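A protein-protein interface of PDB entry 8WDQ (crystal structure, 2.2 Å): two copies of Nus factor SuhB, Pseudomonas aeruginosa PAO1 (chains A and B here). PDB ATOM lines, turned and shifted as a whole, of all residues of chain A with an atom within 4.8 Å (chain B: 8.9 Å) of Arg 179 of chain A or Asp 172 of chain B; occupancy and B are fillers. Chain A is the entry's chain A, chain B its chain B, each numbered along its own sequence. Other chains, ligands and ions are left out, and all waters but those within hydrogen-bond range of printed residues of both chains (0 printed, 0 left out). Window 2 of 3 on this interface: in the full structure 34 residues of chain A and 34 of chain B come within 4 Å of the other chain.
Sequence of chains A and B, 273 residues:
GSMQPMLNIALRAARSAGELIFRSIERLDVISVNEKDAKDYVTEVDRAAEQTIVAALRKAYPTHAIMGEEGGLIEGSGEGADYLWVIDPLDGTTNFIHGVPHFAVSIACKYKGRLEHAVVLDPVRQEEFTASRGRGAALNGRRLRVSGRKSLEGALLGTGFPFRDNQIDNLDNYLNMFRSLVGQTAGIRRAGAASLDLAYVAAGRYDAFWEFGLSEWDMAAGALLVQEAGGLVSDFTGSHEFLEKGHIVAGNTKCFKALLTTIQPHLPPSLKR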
ATOM      1  N   LEU A 175       6.919  24.847  10.161  1.00  0.00           N
ATOM      2  CA  LEU A 175       8.246  24.376   9.791  1.00  0.00           C
ATOM      3  C   LEU A 175       8.507  24.619   8.314  1.00  0.00           C
ATOM      4  O   LEU A 175       9.663  24.778   7.908  1.00  0.00           O
ATOM      5  CB  LEU A 175       8.411  22.900  10.153  1.00  0.00           C
ATOM      6  CG  LEU A 175       8.486  22.632  11.663  1.00  0.00           C
ATOM      7  CD1 LEU A 175       8.568  21.141  11.986  1.00  0.00           C
ATOM      8  CD2 LEU A 175       9.660  23.376  12.282  1.00  0.00           C
ATOM      9  N   ASN A 176       7.444  24.692   7.507  1.00  0.00           N
ATOM     10  CA  ASN A 176       7.618  25.055   6.108  1.00  0.00           C
ATOM     11  C   ASN A 176       7.996  26.526   5.981  1.00  0.00           C
ATOM     12  O   ASN A 176       8.951  26.869   5.268  1.00  0.00           O
ATOM     13  CB  ASN A 176       6.345  24.739   5.321  1.00  0.00           C
ATOM     14  CG  ASN A 176       6.211  23.256   5.013  1.00  0.00           C
ATOM     15  OD1 ASN A 176       7.211  22.565   4.803  1.00  0.00           O
ATOM     16  ND2 ASN A 176       4.974  22.758   4.992  1.00  0.00           N
ATOM     17  N   MET A 177       7.281  27.405   6.698  1.00  0.00           N
ATOM     18  CA  MET A 177       7.653  28.816   6.727  1.00  0.00           C
ATOM     19  C   MET A 177       9.136  28.944   7.035  1.00  0.00           C
ATOM     20  O   MET A 177       9.937  29.359   6.183  1.00  0.00           O
ATOM     21  CB  MET A 177       6.824  29.577   7.774  1.00  0.00           C
ATOM     22  CG  MET A 177       5.302  29.505   7.606  1.00  0.00           C
ATOM     23  SD  MET A 177       4.386  30.431   8.880  1.00  0.00           S
ATOM     24  CE  MET A 177       2.951  29.387   9.141  1.00  0.00           C
ATOM     25  N   PHE A 178       9.514  28.516   8.245  1.00  0.00           N
ATOM     26  CA  PHE A 178      10.908  28.458   8.667  1.00  0.00           C
ATOM     27  C   PHE A 178      11.826  27.986   7.546  1.00  0.00           C
ATOM     28  O   PHE A 178      12.828  28.640   7.235  1.00  0.00           O
ATOM     29  CB  PHE A 178      11.020  27.532   9.880  1.00  0.00           C
ATOM     30  CG  PHE A 178      12.336  27.615  10.591  1.00  0.00           C
ATOM     31  CD1 PHE A 178      13.445  26.933  10.109  1.00  0.00           C
ATOM     32  CD2 PHE A 178      12.462  28.361  11.754  1.00  0.00           C
ATOM     33  CE1 PHE A 178      14.659  26.995  10.767  1.00  0.00           C
ATOM     34  CE2 PHE A 178      13.675  28.430  12.418  1.00  0.00           C
ATOM     35  CZ  PHE A 178      14.775  27.746  11.925  1.00  0.00           C
ATOM     36  N   ARG A 179      11.470  26.874   6.898  1.00  0.00           N
ATOM     37  CA  ARG A 179      12.359  26.288   5.899  1.00  0.00           C
ATOM     38  C   ARG A 179      12.669  27.293   4.798  1.00  0.00           C
ATOM     39  O   ARG A 179      13.839  27.609   4.538  1.00  0.00           O
ATOM     40  CB  ARG A 179      11.731  25.012   5.330  1.00  0.00           C
ATOM     41  CG  ARG A 179      12.381  24.464   4.059  1.00  0.00           C
ATOM     42  CD  ARG A 179      12.194  22.951   3.955  1.00  0.00           C
ATOM     43  NE  ARG A 179      10.933  22.510   4.544  1.00  0.00           N
ATOM     44  CZ  ARG A 179      10.759  21.356   5.178  1.00  0.00           C
ATOM     45  NH1 ARG A 179      11.746  20.480   5.306  1.00  0.00           N
ATOM     46  NH2 ARG A 179       9.569  21.074   5.702  1.00  0.00           N
ATOM     47  N   SER A 180      11.625  27.873   4.199  1.00  0.00           N
ATOM     48  CA  SER A 180      11.810  28.793   3.083  1.00  0.00           C
ATOM     49  C   SER A 180      12.562  30.061   3.472  1.00  0.00           C
ATOM     50  O   SER A 180      12.893  30.856   2.588  1.00  0.00           O
ATOM     51  CB  SER A 180      10.450  29.161   2.486  1.00  0.00           C
ATOM     52  OG  SER A 180       9.621  29.760   3.470  1.00  0.00           O
ATOM     53  N   LEU A 181      12.838  30.274   4.759  1.00  0.00           N
ATOM     54  CA  LEU A 181      13.567  31.464   5.167  1.00  0.00           C
ATOM     55  C   LEU A 181      15.035  31.198   5.455  1.00  0.00           C
ATOM     56  O   LEU A 181      15.790  32.156   5.649  1.00  0.00           O
ATOM     57  CB  LEU A 181      12.914  32.089   6.404  1.00  0.00           C
ATOM     58  CG  LEU A 181      11.508  32.642   6.173  1.00  0.00           C
ATOM     59  CD1 LEU A 181      10.726  32.678   7.482  1.00  0.00           C
ATOM     60  CD2 LEU A 181      11.564  34.025   5.517  1.00  0.00           C
ATOM     61  N   VAL A 182      15.464  29.935   5.471  1.00  0.00           N
ATOM     62  CA  VAL A 182      16.809  29.636   5.953  1.00  0.00           C
ATOM     63  C   VAL A 182      17.860  30.064   4.930  1.00  0.00           C
ATOM     64  O   VAL A 182      18.948  30.528   5.296  1.00  0.00           O
ATOM     65  CB  VAL A 182      16.920  28.143   6.314  1.00  0.00           C
ATOM     66  CG1 VAL A 182      18.373  27.677   6.297  1.00  0.00           C
ATOM     67  CG2 VAL A 182      16.286  27.887   7.676  1.00  0.00           C
ATOM     68  N   GLY A 183      17.549  29.941   3.639  1.00  0.00           N
ATOM     69  CA  GLY A 183      18.555  30.215   2.622  1.00  0.00           C
ATOM     70  C   GLY A 183      18.996  31.667   2.584  1.00  0.00           C
ATOM     71  O   GLY A 183      20.192  31.969   2.654  1.00  0.00           O
ATOM     72  N   PRO B 162      20.755  24.864  11.391  1.00  0.00           N
ATOM     73  CA  PRO B 162      21.734  24.655  10.299  1.00  0.00           C
ATOM     74  C   PRO B 162      21.555  25.685   9.185  1.00  0.00           C
ATOM     75  O   PRO B 162      20.929  25.449   8.148  1.00  0.00           O
ATOM     76  CB  PRO B 162      21.420  23.231   9.836  1.00  0.00           C
ATOM     77  CG  PRO B 162      19.951  23.043  10.141  1.00  0.00           C
ATOM     78  CD  PRO B 162      19.575  23.991  11.259  1.00  0.00           C
ATOM     79  N   GLN B 167      25.015  23.217   4.803  1.00  0.00           N
ATOM     80  CA  GLN B 167      24.144  22.393   5.627  1.00  0.00           C
ATOM     81  C   GLN B 167      22.778  22.168   4.984  1.00  0.00           C
ATOM     82  O   GLN B 167      21.904  21.555   5.611  1.00  0.00           O
ATOM     83  CB  GLN B 167      23.977  23.021   7.014  1.00  0.00           C
ATOM     84  CG  GLN B 167      25.291  23.397   7.691  1.00  0.00           C
ATOM     85  CD  GLN B 167      25.095  24.055   9.045  1.00  0.00           C
ATOM     86  OE1 GLN B 167      24.683  25.213   9.134  1.00  0.00           O
ATOM     87  NE2 GLN B 167      25.401  23.323  10.107  1.00  0.00           N
ATOM     88  N   ILE B 168      22.588  22.625   3.740  1.00  0.00           N
ATOM     89  CA  ILE B 168      21.256  22.626   3.131  1.00  0.00           C
ATOM     90  C   ILE B 168      20.689  21.211   3.059  1.00  0.00           C
ATOM     91  O   ILE B 168      19.529  20.972   3.421  1.00  0.00           O
ATOM     92  CB  ILE B 168      21.297  23.305   1.747  1.00  0.00           C
ATOM     93  CG1 ILE B 168      19.882  23.526   1.207  1.00  0.00           C
ATOM     94  CG2 ILE B 168      22.159  22.525   0.744  1.00  0.00           C
ATOM     95  CD1 ILE B 168      18.968  24.254   2.163  1.00  0.00           C
ATOM     96  N   ASP B 169      21.506  20.241   2.631  1.00  0.00           N
ATOM     97  CA  ASP B 169      21.040  18.864   2.500  1.00  0.00           C
ATOM     98  C   ASP B 169      20.751  18.207   3.842  1.00  0.00           C
ATOM     99  O   ASP B 169      20.192  17.104   3.865  1.00  0.00           O
ATOM    100  CB  ASP B 169      22.063  18.025   1.729  1.00  0.00           C
ATOM    101  CG  ASP B 169      22.091  18.354   0.246  1.00  0.00           C
ATOM    102  OD1 ASP B 169      21.131  18.988  -0.242  1.00  0.00           O
ATOM    103  OD2 ASP B 169      23.064  17.962  -0.434  1.00  0.00           O
ATOM    104  N   ASN B 170      21.122  18.843   4.946  1.00  0.00           N
ATOM    105  CA  ASN B 170      20.779  18.352   6.268  1.00  0.00           C
ATOM    106  C   ASN B 170      19.566  19.063   6.853  1.00  0.00           C
ATOM    107  O   ASN B 170      19.007  18.586   7.849  1.00  0.00           O
ATOM    108  CB  ASN B 170      21.979  18.511   7.205  1.00  0.00           C
ATOM    109  CG  ASN B 170      23.141  17.611   6.821  1.00  0.00           C
ATOM    110  OD1 ASN B 170      23.022  16.766   5.932  1.00  0.00           O
ATOM    111  ND2 ASN B 170      24.278  17.798   7.485  1.00  0.00           N
ATOM    112  N   LEU B 171      19.132  20.160   6.224  1.00  0.00           N
ATOM    113  CA  LEU B 171      18.074  20.998   6.781  1.00  0.00           C
ATOM    114  C   LEU B 171      16.835  20.174   7.115  1.00  0.00           C
ATOM    115  O   LEU B 171      16.353  20.192   8.256  1.00  0.00           O
ATOM    116  CB  LEU B 171      17.736  22.114   5.788  1.00  0.00           C
ATOM    117  CG  LEU B 171      17.171  23.463   6.253  1.00  0.00           C
ATOM    118  CD1 LEU B 171      16.814  24.323   5.042  1.00  0.00           C
ATOM    119  CD2 LEU B 171      15.991  23.348   7.196  1.00  0.00           C
ATOM    120  N   ASP B 172      16.318  19.430   6.131  1.00  0.00           N
ATOM    121  CA  ASP B 172      15.158  18.575   6.367  1.00  0.00           C
ATOM    122  C   ASP B 172      15.393  17.630   7.538  1.00  0.00           C
ATOM    123  O   ASP B 172      14.558  17.544   8.448  1.00  0.00           O
ATOM    124  CB  ASP B 172      14.802  17.796   5.100  1.00  0.00           C
ATOM    125  CG  ASP B 172      14.183  18.678   4.026  1.00  0.00           C
ATOM    126  OD1 ASP B 172      14.026  19.895   4.275  1.00  0.00           O
ATOM    127  OD2 ASP B 172      13.837  18.152   2.945  1.00  0.00           O
ATOM    128  N   ASN B 173      16.538  16.937   7.554  1.00  0.00           N
ATOM    129  CA  ASN B 173      16.835  16.058   8.683  1.00  0.00           C
ATOM    130  C   ASN B 173      16.694  16.815   9.992  1.00  0.00           C
ATOM    131  O   ASN B 173      16.002  16.367  10.917  1.00  0.00           O
ATOM    132  CB  ASN B 173      18.237  15.463   8.563  1.00  0.00           C
ATOM    133  CG  ASN B 173      18.358  14.490   7.423  1.00  0.00           C
ATOM    134  OD1 ASN B 173      17.768  13.412   7.454  1.00  0.00           O
ATOM    135  ND2 ASN B 173      19.134  14.857   6.406  1.00  0.00           N
ATOM    136  N   TYR B 174      17.295  18.005  10.055  1.00  0.00           N
ATOM    137  CA  TYR B 174      17.209  18.801  11.269  1.00  0.00           C
ATOM    138  C   TYR B 174      15.757  19.095  11.615  1.00  0.00           C
ATOM    139  O   TYR B 174      15.322  18.879  12.754  1.00  0.00           O
ATOM    140  CB  TYR B 174      17.989  20.102  11.112  1.00  0.00           C
ATOM    141  CG  TYR B 174      17.927  20.934  12.362  1.00  0.00           C
ATOM    142  CD1 TYR B 174      18.753  20.659  13.444  1.00  0.00           C
ATOM    143  CD2 TYR B 174      16.993  21.952  12.488  1.00  0.00           C
ATOM    144  CE1 TYR B 174      18.685  21.412  14.599  1.00  0.00           C
ATOM    145  CE2 TYR B 174      16.908  22.705  13.639  1.00  0.00           C
ATOM    146  CZ  TYR B 174      17.754  22.428  14.691  1.00  0.00           C
ATOM    147  OH  TYR B 174      17.667  23.172  15.834  1.00  0.00           O
ATOM    148  N   LEU B 175      14.980  19.559  10.631  1.00  0.00           N
ATOM    149  CA  LEU B 175      13.594  19.906  10.920  1.00  0.00           C
ATOM    150  C   LEU B 175      12.805  18.672  11.326  1.00  0.00           C
ATOM    151  O   LEU B 175      11.830  18.775  12.081  1.00  0.00           O
ATOM    152  CB  LEU B 175      12.946  20.597   9.718  1.00  0.00           C
ATOM    153  CG  LEU B 175      13.441  22.008   9.383  1.00  0.00           C
ATOM    154  CD1 LEU B 175      12.677  22.581   8.194  1.00  0.00           C
ATOM    155  CD2 LEU B 175      13.343  22.934  10.587  1.00  0.00           C
ATOM    156  N   ASN B 176      13.231  17.494  10.865  1.00  0.00           N
ATOM    157  CA  ASN B 176      12.616  16.267  11.350  1.00  0.00           C
ATOM    158  C   ASN B 176      12.961  16.051  12.817  1.00  0.00           C
ATOM    159  O   ASN B 176      12.063  15.853  13.646  1.00  0.00           O
ATOM    160  CB  ASN B 176      13.054  15.081  10.487  1.00  0.00           C
ATOM    161  CG  ASN B 176      12.214  14.941   9.229  1.00  0.00           C
ATOM    162  OD1 ASN B 176      11.093  15.448   9.166  1.00  0.00           O
ATOM    163  ND2 ASN B 176      12.749  14.252   8.221  1.00  0.00           N
ATOM    164  N   MET B 177      14.254  16.139  13.160  1.00  0.00           N
ATOM    165  CA  MET B 177      14.676  16.070  14.557  1.00  0.00           C
ATOM    166  C   MET B 177      13.829  17.009  15.406  1.00  0.00           C
ATOM    167  O   MET B 177      13.080  16.578  16.294  1.00  0.00           O
ATOM    168  CB  MET B 177      16.158  16.452  14.691  1.00  0.00           C
ATOM    169  CG  MET B 177      17.185  15.420  14.243  1.00  0.00           C
ATOM    170  SD  MET B 177      18.860  16.131  14.232  1.00  0.00           S
ATOM    171  CE  MET B 177      19.369  15.906  12.529  1.00  0.00           C
ATOM    172  N   PHE B 178      13.926  18.305  15.097  1.00  0.00           N
ATOM    173  CA  PHE B 178      13.148  19.342  15.761  1.00  0.00           C
ATOM    174  C   PHE B 178      11.696  18.928  15.941  1.00  0.00           C
ATOM    175  O   PHE B 178      11.152  19.015  17.049  1.00  0.00           O
ATOM    176  CB  PHE B 178      13.245  20.644  14.955  1.00  0.00           C
ATOM    177  CG  PHE B 178      12.650  21.842  15.648  1.00  0.00           C
ATOM    178  CD1 PHE B 178      11.281  22.076  15.617  1.00  0.00           C
ATOM    179  CD2 PHE B 178      13.465  22.744  16.312  1.00  0.00           C
ATOM    180  CE1 PHE B 178      10.732  23.179  16.247  1.00  0.00           C
ATOM    181  CE2 PHE B 178      12.924  23.855  16.944  1.00  0.00           C
ATOM    182  CZ  PHE B 178      11.554  24.071  16.910  1.00  0.00           C
ATOM    183  N   ARG B 179      11.060  18.432  14.873  1.00  0.00           N
ATOM    184  CA  ARG B 179       9.633  18.143  14.973  1.00  0.00           C
ATOM    185  C   ARG B 179       9.372  17.109  16.056  1.00  0.00           C
ATOM    186  O   ARG B 179       8.506  17.299  16.920  1.00  0.00           O
ATOM    187  CB  ARG B 179       9.073  17.665  13.635  1.00  0.00           C
ATOM    188  CG  ARG B 179       7.545  17.755  13.573  1.00  0.00           C
ATOM    189  CD  ARG B 179       6.945  16.677  12.687  1.00  0.00           C
ATOM    190  NE  ARG B 179       5.508  16.845  12.498  1.00  0.00           N
ATOM    191  CZ  ARG B 179       4.569  16.223  13.202  1.00  0.00           C
ATOM    192  NH1 ARG B 179       4.876  15.398  14.193  1.00  0.00           N
ATOM    193  NH2 ARG B 179       3.290  16.430  12.902  1.00  0.00           N
ATOM    194  N   PHE B 212      24.887  20.630  14.808  1.00  0.00           N
ATOM    195  CA  PHE B 212      25.976  20.178  13.954  1.00  0.00           C
ATOM    196  C   PHE B 212      26.502  21.355  13.140  1.00  0.00           C
ATOM    197  O   PHE B 212      25.889  22.424  13.077  1.00  0.00           O
ATOM    198  CB  PHE B 212      25.555  19.012  13.043  1.00  0.00           C
ATOM    199  CG  PHE B 212      24.461  19.346  12.073  1.00  0.00           C
ATOM    200  CD1 PHE B 212      23.131  19.188  12.429  1.00  0.00           C
ATOM    201  CD2 PHE B 212      24.760  19.788  10.795  1.00  0.00           C
ATOM    202  CE1 PHE B 212      22.118  19.483  11.535  1.00  0.00           C
ATOM    203  CE2 PHE B 212      23.752  20.086   9.897  1.00  0.00           C
ATOM    204  CZ  PHE B 212      22.431  19.933  10.270  1.00  0.00           C
ATOM    205  N   HIS B 266      17.281  10.136  12.423  1.00  0.00           N
ATOM    206  CA  HIS B 266      17.406  11.184  11.415  1.00  0.00           C
ATOM    207  C   HIS B 266      18.851  11.403  10.976  1.00  0.00           C
ATOM    208  O   HIS B 266      19.165  12.437  10.377  1.00  0.00           O
ATOM    209  CB  HIS B 266      16.797  12.485  11.934  1.00  0.00           C
ATOM    210  CG  HIS B 266      15.464  12.303  12.587  1.00  0.00           C
ATOM    211  ND1 HIS B 266      14.294  12.184  11.868  1.00  0.00           N
ATOM    212  CD2 HIS B 266      15.114  12.209  13.892  1.00  0.00           C
ATOM    213  CE1 HIS B 266      13.281  12.028  12.701  1.00  0.00           C
ATOM    214  NE2 HIS B 266      13.751  12.041  13.936  1.00  0.00           N
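Of chain A, only Arg 179 comes within 4 Å of Asp 172 of chain B. Of the printed residues of chain A, Pro 162 of chain B touches Val 182 (3.9 Å). Of the printed residues of chain A, Leu 171 of chain B touches Val 182 (3.9 Å). Of the printed residues of chain A, Leu 175 of chain B touches Leu 175 and Arg 179. Printed residues of chain B within 4 Å of Leu 175 of chain A: Leu 175 (3.7 Å), Phe 178 (3.9 Å) and Arg 179 (3.9 Å). Of the printed residues of chain A, Phe 178 of chain B touches Leu 175 (3.9 Å).
Leu 175 of chain B touches its own counterpart, Leu 175 of chain A. Leu 175 of chain A touches Phe 178 of chain B, but with the chains exchanged Phe 178 of chain A does not touch Leu 175 of chain B (4.03 Å). Leu 175 of chain A touches Arg 179 of chain B, and with the chains exchanged Arg 179 of chain A touches Leu 175 of chain B.
NH1 of Arg 179 of chain A is in salt-bridge range of OD1 of Asp 172 of chain B (2.6 Å).
Hydrophobic or aromatic side chains of chain A within 4 Å of the printed part of chain B: Leu 175 and Val 182. Hydrophobic or aromatic side chains of chain B that line the printed part of chain A: Leu 171, Leu 175 and Phe 178. Among the printed residues, 7 pairs touch across the chains. Among the printed residues, Asp or Glu carboxylates within 4 Å of a Lys or Arg side-chain nitrogen of the other chain: Arg 179 of chain A with Asp 172 of chain B (2.6 Å).
OD1 of Asn 176 of chain A sits at hydrogen-bond distance from NH2 of Arg 179 of chain A (2.9 Å).
Leu 175 of chain B touches Leu 175 of chain A. Phe 178 of chain B touches Leu 175 of chain A. CD1 of Leu 175 of chain A touches CG of Arg 179 of chain B (3.9 Å). Arg 179 of chain A touches Leu 175 of chain B (NH1 to CD1, 3.7 Å). Val 182 of chain A touches Pro 162 of chain B (CG1 to O, 3.9 Å). Val 182 of chain A touches Leu 171 of chain B (CG1 to CD1, 3.9 Å).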
